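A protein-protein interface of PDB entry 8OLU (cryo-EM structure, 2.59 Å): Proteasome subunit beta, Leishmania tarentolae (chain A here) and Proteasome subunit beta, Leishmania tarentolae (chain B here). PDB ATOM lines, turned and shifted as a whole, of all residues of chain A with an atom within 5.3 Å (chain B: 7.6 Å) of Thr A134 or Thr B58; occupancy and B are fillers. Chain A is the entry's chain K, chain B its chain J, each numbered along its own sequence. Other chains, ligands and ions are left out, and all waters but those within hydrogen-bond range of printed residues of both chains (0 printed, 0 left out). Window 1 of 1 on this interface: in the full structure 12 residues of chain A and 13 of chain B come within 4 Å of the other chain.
O of Leu A135 is in hydrogen-bond range of NE2 of Gln B61 (2.8 Å). The side-chain carboxylate of Glu B30 lies close to the side-chain carboxylate of Asp A130, at 3.1 Å. The side-chain amide oxygen (OE1) of Gln B61 lies close to the backbone carbonyl oxygen (O) of Gly A133, 3.5 Å away. The side-chain hydroxyl (OG1) of Thr B58 sits at hydrogen-bond distance from the guanidinium group (NH2) of Arg A87 (3.0 Å). The guanidinium group (NH1) of Arg A87 sits at hydrogen-bond distance from the side-chain hydroxyl (OG1) of Thr B62 (2.7 Å). The side-chain hydroxyl of Thr B58 is in hydrogen-bond range of the backbone carbonyl oxygen of Leu A132 (2.8 Å). The backbone carbonyl oxygen (O) of Gly A133 sits at hydrogen-bond distance from the side-chain hydroxyl (OG1) of Thr B58, 3.3 Å away. OE1 of Glu B30 sits at hydrogen-bond distance from OH of Tyr A128 (2.4 Å).
Of the 11 printed residues of chain A, 10 touch a printed residue of chain B.
The side-chain hydroxyl of Thr A134 lies within hydrogen-bond range of the side-chain carboxylate of Asp A130, at 3.2 Å. The backbone NH of Arg B57 is in hydrogen-bond range of the side-chain hydroxyl of Ser B7, at 2.8 Å. O of Thr B58 lies within hydrogen-bond range of OG1 of Thr B62, 3.0 Å away. O of Gln A136 lies within hydrogen-bond range of N of Tyr A128 (2.8 Å). The side-chain carboxylate (OD1) of Asp A130 sits at hydrogen-bond distance from the backbone NH (N) of Leu A132 (2.8 Å). The side-chain carboxylate (OD1) of Asp A130 is in hydrogen-bond range of the backbone NH (N) of Gly A133 (3.3 Å).
Among the printed residues, pairs that only touch across the chains: Thr A134 with Arg B57 (3.5 Å), Thr A134 with Gln B61 (3.5 Å), Arg A87 with Gln B61 (3.7 Å), Ala A91 with Thr B58 (3.8 Å), Thr A134 with Thr B58 (3.8 Å), Ala A91 with Thr B62 (3.8 Å), Ile A94 with Thr B58 (3.8 Å), Tyr A128 with Ile B35 (3.8 Å) and Gln A136 with Leu B28 (3.9 Å).
Of chain B, only Arg B57, Thr B58 and Gln B61 come within 4 Å of Thr A134. Printed residues of chain A within 4 Å of Glu B30: Tyr A128 and Asp A130. Of the printed residues of chain A, Arg B57 touches Thr A134. Thr B58 touches just these residues of chain A: Arg A87 (3.0 Å), Ala A91 (3.8 Å), Ile A94 (3.8 Å), Leu A132 (2.8 Å), Gly A133 (3.3 Å) and Thr A134 (3.8 Å). The nearest residue of chain B that does not touch Thr A134 is Leu B28 (4.3 Å). The nearest printed residue of chain A that does not touch Thr B58 is Asp A130 (5.6 Å). The nearest printed residue of chain B that does not touch Leu A135 is Arg B57 (5.1 Å).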
ATOM      1  N   ARG A  87      -4.812 -20.428  25.201  1.00  0.00           N
ATOM      2  CA  ARG A  87      -3.480 -19.975  25.505  1.00  0.00           C
ATOM      3  C   ARG A  87      -2.508 -20.401  24.439  1.00  0.00           C
ATOM      4  O   ARG A  87      -1.647 -19.656  24.089  1.00  0.00           O
ATOM      5  CB  ARG A  87      -2.943 -20.570  26.799  1.00  0.00           C
ATOM      6  CG  ARG A  87      -1.688 -19.834  27.232  1.00  0.00           C
ATOM      7  CD  ARG A  87      -0.846 -20.695  28.106  1.00  0.00           C
ATOM      8  NE  ARG A  87       0.007 -21.578  27.331  1.00  0.00           N
ATOM      9  CZ  ARG A  87       1.119 -21.137  26.829  1.00  0.00           C
ATOM     10  NH1 ARG A  87       1.896 -21.943  26.160  1.00  0.00           N
ATOM     11  NH2 ARG A  87       1.391 -19.858  26.974  1.00  0.00           N
ATOM     12  N   ALA A  91      -0.234 -18.093  22.189  1.00  0.00           N
ATOM     13  CA  ALA A  91       1.207 -18.184  22.336  1.00  0.00           C
ATOM     14  C   ALA A  91       1.853 -18.474  21.006  1.00  0.00           C
ATOM     15  O   ALA A  91       2.945 -18.021  20.718  1.00  0.00           O
ATOM     16  CB  ALA A  91       1.571 -19.305  23.254  1.00  0.00           C
ATOM     17  N   ILE A  94       2.518 -15.603  18.815  1.00  0.00           N
ATOM     18  CA  ILE A  94       3.486 -14.520  18.950  1.00  0.00           C
ATOM     19  C   ILE A  94       4.769 -14.865  18.224  1.00  0.00           C
ATOM     20  O   ILE A  94       5.604 -14.004  18.023  1.00  0.00           O
ATOM     21  CB  ILE A  94       3.792 -14.153  20.400  1.00  0.00           C
ATOM     22  CG1 ILE A  94       4.746 -15.162  21.032  1.00  0.00           C
ATOM     23  CG2 ILE A  94       2.498 -14.000  21.162  1.00  0.00           C
ATOM     24  CD1 ILE A  94       4.696 -15.163  22.524  1.00  0.00           C
ATOM     25  N   TYR A 128      -7.265 -15.301  33.537  1.00  0.00           N
ATOM     26  CA  TYR A 128      -6.732 -14.134  32.917  1.00  0.00           C
ATOM     27  C   TYR A 128      -5.798 -14.544  31.821  1.00  0.00           C
ATOM     28  O   TYR A 128      -4.957 -15.353  32.079  1.00  0.00           O
ATOM     29  CB  TYR A 128      -6.036 -13.408  34.016  1.00  0.00           C
ATOM     30  CG  TYR A 128      -5.258 -12.231  33.552  1.00  0.00           C
ATOM     31  CD1 TYR A 128      -3.965 -12.370  33.064  1.00  0.00           C
ATOM     32  CD2 TYR A 128      -5.780 -10.979  33.714  1.00  0.00           C
ATOM     33  CE1 TYR A 128      -3.263 -11.290  32.583  1.00  0.00           C
ATOM     34  CE2 TYR A 128      -5.047  -9.884  33.319  1.00  0.00           C
ATOM     35  CZ  TYR A 128      -3.808 -10.042  32.735  1.00  0.00           C
ATOM     36  OH  TYR A 128      -3.145  -8.890  32.358  1.00  0.00           O
ATOM     37  N   MET A 129      -6.018 -14.087  30.594  1.00  0.00           N
ATOM     38  CA  MET A 129      -5.062 -14.284  29.542  1.00  0.00           C
ATOM     39  C   MET A 129      -4.586 -12.959  29.052  1.00  0.00           C
ATOM     40  O   MET A 129      -5.314 -12.015  29.181  1.00  0.00           O
ATOM     41  CB  MET A 129      -5.691 -14.917  28.348  1.00  0.00           C
ATOM     42  CG  MET A 129      -5.661 -16.344  28.525  1.00  0.00           C
ATOM     43  SD  MET A 129      -6.600 -17.162  27.245  1.00  0.00           S
ATOM     44  CE  MET A 129      -7.907 -17.737  28.325  1.00  0.00           C
ATOM     45  N   ASP A 130      -3.381 -12.897  28.509  1.00  0.00           N
ATOM     46  CA  ASP A 130      -2.961 -11.711  27.807  1.00  0.00           C
ATOM     47  C   ASP A 130      -2.541 -12.138  26.418  1.00  0.00           C
ATOM     48  O   ASP A 130      -2.455 -13.306  26.104  1.00  0.00           O
ATOM     49  CB  ASP A 130      -1.932 -10.961  28.630  1.00  0.00           C
ATOM     50  CG  ASP A 130      -0.487 -11.459  28.551  1.00  0.00           C
ATOM     51  OD1 ASP A 130      -0.175 -12.257  27.599  1.00  0.00           O
ATOM     52  OD2 ASP A 130       0.359 -11.011  29.447  1.00  0.00           O
ATOM     53  N   LEU A 132      -0.021 -12.410  24.824  1.00  0.00           N
ATOM     54  CA  LEU A 132       1.124 -13.234  24.572  1.00  0.00           C
ATOM     55  C   LEU A 132       0.901 -14.670  24.970  1.00  0.00           C
ATOM     56  O   LEU A 132       1.738 -15.524  24.735  1.00  0.00           O
ATOM     57  CB  LEU A 132       2.249 -12.725  25.423  1.00  0.00           C
ATOM     58  CG  LEU A 132       2.680 -11.296  25.175  1.00  0.00           C
ATOM     59  CD1 LEU A 132       3.309 -10.722  26.459  1.00  0.00           C
ATOM     60  CD2 LEU A 132       3.659 -11.249  24.034  1.00  0.00           C
ATOM     61  N   GLY A 133      -0.181 -14.920  25.666  1.00  0.00           N
ATOM     62  CA  GLY A 133      -0.551 -16.264  26.022  1.00  0.00           C
ATOM     63  C   GLY A 133      -0.119 -16.536  27.433  1.00  0.00           C
ATOM     64  O   GLY A 133       0.188 -17.644  27.825  1.00  0.00           O
ATOM     65  N   THR A 134      -0.111 -15.514  28.214  1.00  0.00           N
ATOM     66  CA  THR A 134       0.000 -15.764  29.610  1.00  0.00           C
ATOM     67  C   THR A 134      -1.331 -16.306  30.023  1.00  0.00           C
ATOM     68  O   THR A 134      -2.283 -16.079  29.318  1.00  0.00           O
ATOM     69  CB  THR A 134       0.350 -14.483  30.350  1.00  0.00           C
ATOM     70  OG1 THR A 134       1.603 -13.931  29.893  1.00  0.00           O
ATOM     71  CG2 THR A 134       0.452 -14.845  31.798  1.00  0.00           C
ATOM     72  N   LEU A 135      -1.408 -17.173  31.003  1.00  0.00           N
ATOM     73  CA  LEU A 135      -2.698 -17.738  31.337  1.00  0.00           C
ATOM     74  C   LEU A 135      -2.654 -18.031  32.811  1.00  0.00           C
ATOM     75  O   LEU A 135      -1.854 -18.843  33.213  1.00  0.00           O
ATOM     76  CB  LEU A 135      -2.972 -19.032  30.564  1.00  0.00           C
ATOM     77  CG  LEU A 135      -4.123 -19.855  31.174  1.00  0.00           C
ATOM     78  CD1 LEU A 135      -5.436 -19.174  30.904  1.00  0.00           C
ATOM     79  CD2 LEU A 135      -4.206 -21.289  30.661  1.00  0.00           C
ATOM     80  N   GLN A 136      -3.543 -17.445  33.562  1.00  0.00           N
ATOM     81  CA  GLN A 136      -3.493 -17.592  34.992  1.00  0.00           C
ATOM     82  C   GLN A 136      -4.891 -17.687  35.532  1.00  0.00           C
ATOM     83  O   GLN A 136      -5.672 -16.805  35.327  1.00  0.00           O
ATOM     84  CB  GLN A 136      -2.857 -16.351  35.581  1.00  0.00           C
ATOM     85  CG  GLN A 136      -2.709 -16.386  37.087  1.00  0.00           C
ATOM     86  CD  GLN A 136      -1.991 -17.580  37.614  1.00  0.00           C
ATOM     87  OE1 GLN A 136      -0.981 -17.960  37.039  1.00  0.00           O
ATOM     88  NE2 GLN A 136      -2.541 -18.227  38.632  1.00  0.00           N
ATOM     89  N   TYR B   6       9.606  -8.920  32.393  1.00  0.00           N
ATOM     90  CA  TYR B   6       8.262  -8.434  32.244  1.00  0.00           C
ATOM     91  C   TYR B   6       7.385  -9.104  33.264  1.00  0.00           C
ATOM     92  O   TYR B   6       6.651  -8.438  33.940  1.00  0.00           O
ATOM     93  CB  TYR B   6       7.788  -8.707  30.820  1.00  0.00           C
ATOM     94  CG  TYR B   6       6.419  -8.222  30.489  1.00  0.00           C
ATOM     95  CD1 TYR B   6       6.195  -6.887  30.218  1.00  0.00           C
ATOM     96  CD2 TYR B   6       5.340  -9.079  30.480  1.00  0.00           C
ATOM     97  CE1 TYR B   6       4.917  -6.417  29.929  1.00  0.00           C
ATOM     98  CE2 TYR B   6       4.065  -8.642  30.168  1.00  0.00           C
ATOM     99  CZ  TYR B   6       3.842  -7.300  29.886  1.00  0.00           C
ATOM    100  OH  TYR B   6       2.575  -6.806  29.596  1.00  0.00           O
ATOM    101  N   SER B   7       7.507 -10.409  33.434  1.00  0.00           N
ATOM    102  CA  SER B   7       6.553 -11.175  34.221  1.00  0.00           C
ATOM    103  C   SER B   7       6.999 -11.333  35.659  1.00  0.00           C
ATOM    104  O   SER B   7       6.281 -11.862  36.497  1.00  0.00           O
ATOM    105  CB  SER B   7       6.288 -12.536  33.578  1.00  0.00           C
ATOM    106  OG  SER B   7       5.707 -12.435  32.274  1.00  0.00           O
ATOM    107  N   LEU B  28       3.230 -12.876  39.933  1.00  0.00           N
ATOM    108  CA  LEU B  28       3.188 -12.809  38.492  1.00  0.00           C
ATOM    109  C   LEU B  28       2.776 -11.423  38.074  1.00  0.00           C
ATOM    110  O   LEU B  28       1.757 -10.956  38.467  1.00  0.00           O
ATOM    111  CB  LEU B  28       2.124 -13.787  38.025  1.00  0.00           C
ATOM    112  CG  LEU B  28       1.816 -13.628  36.549  1.00  0.00           C
ATOM    113  CD1 LEU B  28       3.061 -13.875  35.711  1.00  0.00           C
ATOM    114  CD2 LEU B  28       0.720 -14.539  36.053  1.00  0.00           C
ATOM    115  N   GLY B  29       3.537 -10.759  37.256  1.00  0.00           N
ATOM    116  CA  GLY B  29       3.255  -9.375  36.949  1.00  0.00           C
ATOM    117  C   GLY B  29       3.144  -9.174  35.458  1.00  0.00           C
ATOM    118  O   GLY B  29       3.381 -10.088  34.682  1.00  0.00           O
ATOM    119  N   GLU B  30       2.727  -7.978  35.094  1.00  0.00           N
ATOM    120  CA  GLU B  30       3.088  -7.328  33.862  1.00  0.00           C
ATOM    121  C   GLU B  30       3.812  -6.062  34.254  1.00  0.00           C
ATOM    122  O   GLU B  30       3.213  -5.037  34.467  1.00  0.00           O
ATOM    123  CB  GLU B  30       1.834  -6.989  33.098  1.00  0.00           C
ATOM    124  CG  GLU B  30       0.977  -8.217  32.816  1.00  0.00           C
ATOM    125  CD  GLU B  30      -0.371  -8.028  32.113  1.00  0.00           C
ATOM    126  OE1 GLU B  30      -0.875  -9.076  31.587  1.00  0.00           O
ATOM    127  OE2 GLU B  30      -0.924  -6.840  32.068  1.00  0.00           O
ATOM    128  N   ILE B  35      -0.485  -9.205  38.892  1.00  0.00           N
ATOM    129  CA  ILE B  35      -1.654  -9.962  38.464  1.00  0.00           C
ATOM    130  C   ILE B  35      -1.988 -11.054  39.466  1.00  0.00           C
ATOM    131  O   ILE B  35      -3.115 -11.492  39.584  1.00  0.00           O
ATOM    132  CB  ILE B  35      -1.358 -10.702  37.156  1.00  0.00           C
ATOM    133  CG1 ILE B  35      -1.040  -9.774  36.006  1.00  0.00           C
ATOM    134  CG2 ILE B  35      -2.507 -11.603  36.852  1.00  0.00           C
ATOM    135  CD1 ILE B  35      -1.981  -8.536  36.009  1.00  0.00           C
ATOM    136  N   GLY B  55      11.311 -15.749  33.472  1.00  0.00           N
ATOM    137  CA  GLY B  55      11.339 -15.139  32.190  1.00  0.00           C
ATOM    138  C   GLY B  55       9.910 -14.865  31.808  1.00  0.00           C
ATOM    139  O   GLY B  55       9.023 -14.800  32.640  1.00  0.00           O
ATOM    140  N   LEU B  56       9.697 -14.716  30.531  1.00  0.00           N
ATOM    141  CA  LEU B  56       8.437 -14.217  30.122  1.00  0.00           C
ATOM    142  C   LEU B  56       7.440 -15.279  30.463  1.00  0.00           C
ATOM    143  O   LEU B  56       7.627 -16.411  30.140  1.00  0.00           O
ATOM    144  CB  LEU B  56       8.562 -13.984  28.633  1.00  0.00           C
ATOM    145  CG  LEU B  56       7.379 -13.280  28.020  1.00  0.00           C
ATOM    146  CD1 LEU B  56       7.114 -11.984  28.747  1.00  0.00           C
ATOM    147  CD2 LEU B  56       7.655 -13.036  26.568  1.00  0.00           C
ATOM    148  N   ARG B  57       6.403 -14.945  31.161  1.00  0.00           N
ATOM    149  CA  ARG B  57       5.551 -15.985  31.642  1.00  0.00           C
ATOM    150  C   ARG B  57       4.983 -16.808  30.515  1.00  0.00           C
ATOM    151  O   ARG B  57       4.823 -17.984  30.742  1.00  0.00           O
ATOM    152  CB  ARG B  57       4.367 -15.410  32.419  1.00  0.00           C
ATOM    153  CG  ARG B  57       3.362 -16.430  32.936  1.00  0.00           C
ATOM    154  CD  ARG B  57       4.136 -17.262  33.916  1.00  0.00           C
ATOM    155  NE  ARG B  57       3.195 -18.162  34.508  1.00  0.00           N
ATOM    156  CZ  ARG B  57       3.536 -19.267  35.125  1.00  0.00           C
ATOM    157  NH1 ARG B  57       4.803 -19.536  35.342  1.00  0.00           N
ATOM    158  NH2 ARG B  57       2.582 -20.113  35.437  1.00  0.00           N
ATOM    159  N   THR B  58       4.565 -16.231  29.376  1.00  0.00           N
ATOM    160  CA  THR B  58       3.997 -17.088  28.359  1.00  0.00           C
ATOM    161  C   THR B  58       4.998 -18.144  27.938  1.00  0.00           C
ATOM    162  O   THR B  58       4.630 -19.288  27.718  1.00  0.00           O
ATOM    163  CB  THR B  58       3.510 -16.433  27.072  1.00  0.00           C
ATOM    164  OG1 THR B  58       3.084 -17.473  26.190  1.00  0.00           O
ATOM    165  CG2 THR B  58       4.538 -15.618  26.308  1.00  0.00           C
ATOM    166  N   ASP B  59       6.271 -17.788  27.856  1.00  0.00           N
ATOM    167  CA  ASP B  59       7.284 -18.762  27.502  1.00  0.00           C
ATOM    168  C   ASP B  59       7.542 -19.707  28.618  1.00  0.00           C
ATOM    169  O   ASP B  59       7.882 -20.834  28.335  1.00  0.00           O
ATOM    170  CB  ASP B  59       8.584 -18.099  27.108  1.00  0.00           C
ATOM    171  CG  ASP B  59       8.435 -17.494  25.714  1.00  0.00           C
ATOM    172  OD1 ASP B  59       7.284 -17.521  25.155  1.00  0.00           O
ATOM    173  OD2 ASP B  59       9.417 -16.999  25.168  1.00  0.00           O
ATOM    174  N   GLN B  60       7.423 -19.279  29.860  1.00  0.00           N
ATOM    175  CA  GLN B  60       7.519 -20.281  30.895  1.00  0.00           C
ATOM    176  C   GLN B  60       6.468 -21.341  30.665  1.00  0.00           C
ATOM    177  O   GLN B  60       6.730 -22.509  30.744  1.00  0.00           O
ATOM    178  CB  GLN B  60       7.255 -19.723  32.259  1.00  0.00           C
ATOM    179  CG  GLN B  60       8.264 -18.660  32.664  1.00  0.00           C
ATOM    180  CD  GLN B  60       7.850 -18.061  33.997  1.00  0.00           C
ATOM    181  OE1 GLN B  60       7.230 -18.767  34.806  1.00  0.00           O
ATOM    182  NE2 GLN B  60       8.098 -16.756  34.172  1.00  0.00           N
ATOM    183  N   GLN B  61       5.263 -20.924  30.333  1.00  0.00           N
ATOM    184  CA  GLN B  61       4.189 -21.874  30.195  1.00  0.00           C
ATOM    185  C   GLN B  61       4.427 -22.750  28.997  1.00  0.00           C
ATOM    186  O   GLN B  61       4.304 -23.942  29.117  1.00  0.00           O
ATOM    187  CB  GLN B  61       2.855 -21.180  30.154  1.00  0.00           C
ATOM    188  CG  GLN B  61       2.486 -20.681  31.539  1.00  0.00           C
ATOM    189  CD  GLN B  61       1.211 -19.868  31.609  1.00  0.00           C
ATOM    190  OE1 GLN B  61       1.061 -18.813  30.994  1.00  0.00           O
ATOM    191  NE2 GLN B  61       0.267 -20.430  32.341  1.00  0.00           N
ATOM    192  N   THR B  62       4.755 -22.148  27.880  1.00  0.00           N
ATOM    193  CA  THR B  62       4.966 -22.900  26.684  1.00  0.00           C
ATOM    194  C   THR B  62       6.069 -23.908  26.842  1.00  0.00           C
ATOM    195  O   THR B  62       5.946 -25.017  26.426  1.00  0.00           O
ATOM    196  CB  THR B  62       5.304 -22.003  25.522  1.00  0.00           C
ATOM    197  OG1 THR B  62       4.261 -21.061  25.282  1.00  0.00           O
ATOM    198  CG2 THR B  62       5.538 -22.843  24.315  1.00  0.00           C
ATOM    199  N   PHE B  63       7.160 -23.498  27.406  1.00  0.00           N
ATOM    200  CA  PHE B  63       8.324 -24.309  27.497  1.00  0.00           C
ATOM    201  C   PHE B  63       8.107 -25.360  28.541  1.00  0.00           C
ATOM    202  O   PHE B  63       8.567 -26.459  28.383  1.00  0.00           O
ATOM    203  CB  PHE B  63       9.485 -23.467  27.983  1.00  0.00           C
ATOM    204  CG  PHE B  63      10.811 -24.170  27.907  1.00  0.00           C
ATOM    205  CD1 PHE B  63      11.424 -24.367  26.680  1.00  0.00           C
ATOM    206  CD2 PHE B  63      11.414 -24.635  29.032  1.00  0.00           C
ATOM    207  CE1 PHE B  63      12.628 -25.046  26.574  1.00  0.00           C
ATOM    208  CE2 PHE B  63      12.599 -25.328  28.945  1.00  0.00           C
ATOM    209  CZ  PHE B  63      13.202 -25.540  27.722  1.00  0.00           C
ATOM    210  N   ALA B  64       7.478 -25.038  29.634  1.00  0.00           N
ATOM    211  CA  ALA B  64       7.200 -26.076  30.572  1.00  0.00           C
ATOM    212  C   ALA B  64       6.341 -27.156  29.971  1.00  0.00           C
ATOM    213  O   ALA B  64       6.450 -28.287  30.390  1.00  0.00           O
ATOM    214  CB  ALA B  64       6.468 -25.562  31.740  1.00  0.00           C
ATOM    215  N   ASN B  65       5.405 -26.794  29.111  1.00  0.00           N
ATOM    216  CA  ASN B  65       4.609 -27.755  28.457  1.00  0.00           C
ATOM    217  C   ASN B  65       5.434 -28.556  27.464  1.00  0.00           C
ATOM    218  O   ASN B  65       5.226 -29.743  27.338  1.00  0.00           O
ATOM    219  CB  ASN B  65       3.501 -27.075  27.681  1.00  0.00           C
ATOM    220  CG  ASN B  65       2.378 -26.528  28.526  1.00  0.00           C
ATOM    221  OD1 ASN B  65       1.688 -25.587  28.107  1.00  0.00           O
ATOM    222  ND2 ASN B  65       2.269 -27.052  29.738  1.00  0.00           N
ATOM    223  N   TRP B 103      13.463 -18.831  23.486  1.00  0.00           N
ATOM    224  CA  TRP B 103      12.508 -18.865  24.532  1.00  0.00           C
ATOM    225  C   TRP B 103      13.008 -17.960  25.620  1.00  0.00           C
ATOM    226  O   TRP B 103      14.069 -18.153  26.170  1.00  0.00           O
ATOM    227  CB  TRP B 103      12.422 -20.286  25.056  1.00  0.00           C
ATOM    228  CG  TRP B 103      11.907 -21.299  24.098  1.00  0.00           C
ATOM    229  CD1 TRP B 103      12.583 -22.360  23.609  1.00  0.00           C
ATOM    230  CD2 TRP B 103      10.591 -21.381  23.599  1.00  0.00           C
ATOM    231  NE1 TRP B 103      11.809 -23.026  22.731  1.00  0.00           N
ATOM    232  CE2 TRP B 103      10.567 -22.455  22.714  1.00  0.00           C
ATOM    233  CE3 TRP B 103       9.430 -20.616  23.767  1.00  0.00           C
ATOM    234  CZ2 TRP B 103       9.413 -22.814  21.996  1.00  0.00           C
ATOM    235  CZ3 TRP B 103       8.291 -20.953  23.044  1.00  0.00           C
ATOM    236  CH2 TRP B 103       8.293 -22.048  22.167  1.00  0.00           C
ATOM    237  N   PHE B 104      12.203 -17.013  26.020  1.00  0.00           N
ATOM    238  CA  PHE B 104      12.625 -16.133  27.058  1.00  0.00           C
ATOM    239  C   PHE B 104      12.369 -16.793  28.380  1.00  0.00           C
ATOM    240  O   PHE B 104      11.503 -16.362  29.121  1.00  0.00           O
ATOM    241  CB  PHE B 104      11.853 -14.849  26.950  1.00  0.00           C
ATOM    242  CG  PHE B 104      12.251 -14.140  25.711  1.00  0.00           C
ATOM    243  CD1 PHE B 104      13.503 -13.564  25.630  1.00  0.00           C
ATOM    244  CD2 PHE B 104      11.411 -14.121  24.615  1.00  0.00           C
ATOM    245  CE1 PHE B 104      13.904 -12.932  24.473  1.00  0.00           C
ATOM    246  CE2 PHE B 104      11.821 -13.518  23.442  1.00  0.00           C
ATOM    247  CZ  PHE B 104      13.070 -12.929  23.381  1.00  0.00           C
ATOM    248  N   VAL B 105      13.160 -17.787  28.690  1.00  0.00           N
ATOM    249  CA  VAL B 105      13.025 -18.406  29.982  1.00  0.00           C
ATOM    250  C   VAL B 105      14.403 -18.631  30.509  1.00  0.00           C
ATOM    251  O   VAL B 105      15.312 -18.756  29.721  1.00  0.00           O
ATOM    252  CB  VAL B 105      12.331 -19.764  29.904  1.00  0.00           C
ATOM    253  CG1 VAL B 105      10.944 -19.647  29.404  1.00  0.00           C
ATOM    254  CG2 VAL B 105      13.048 -20.720  29.002  1.00  0.00           C
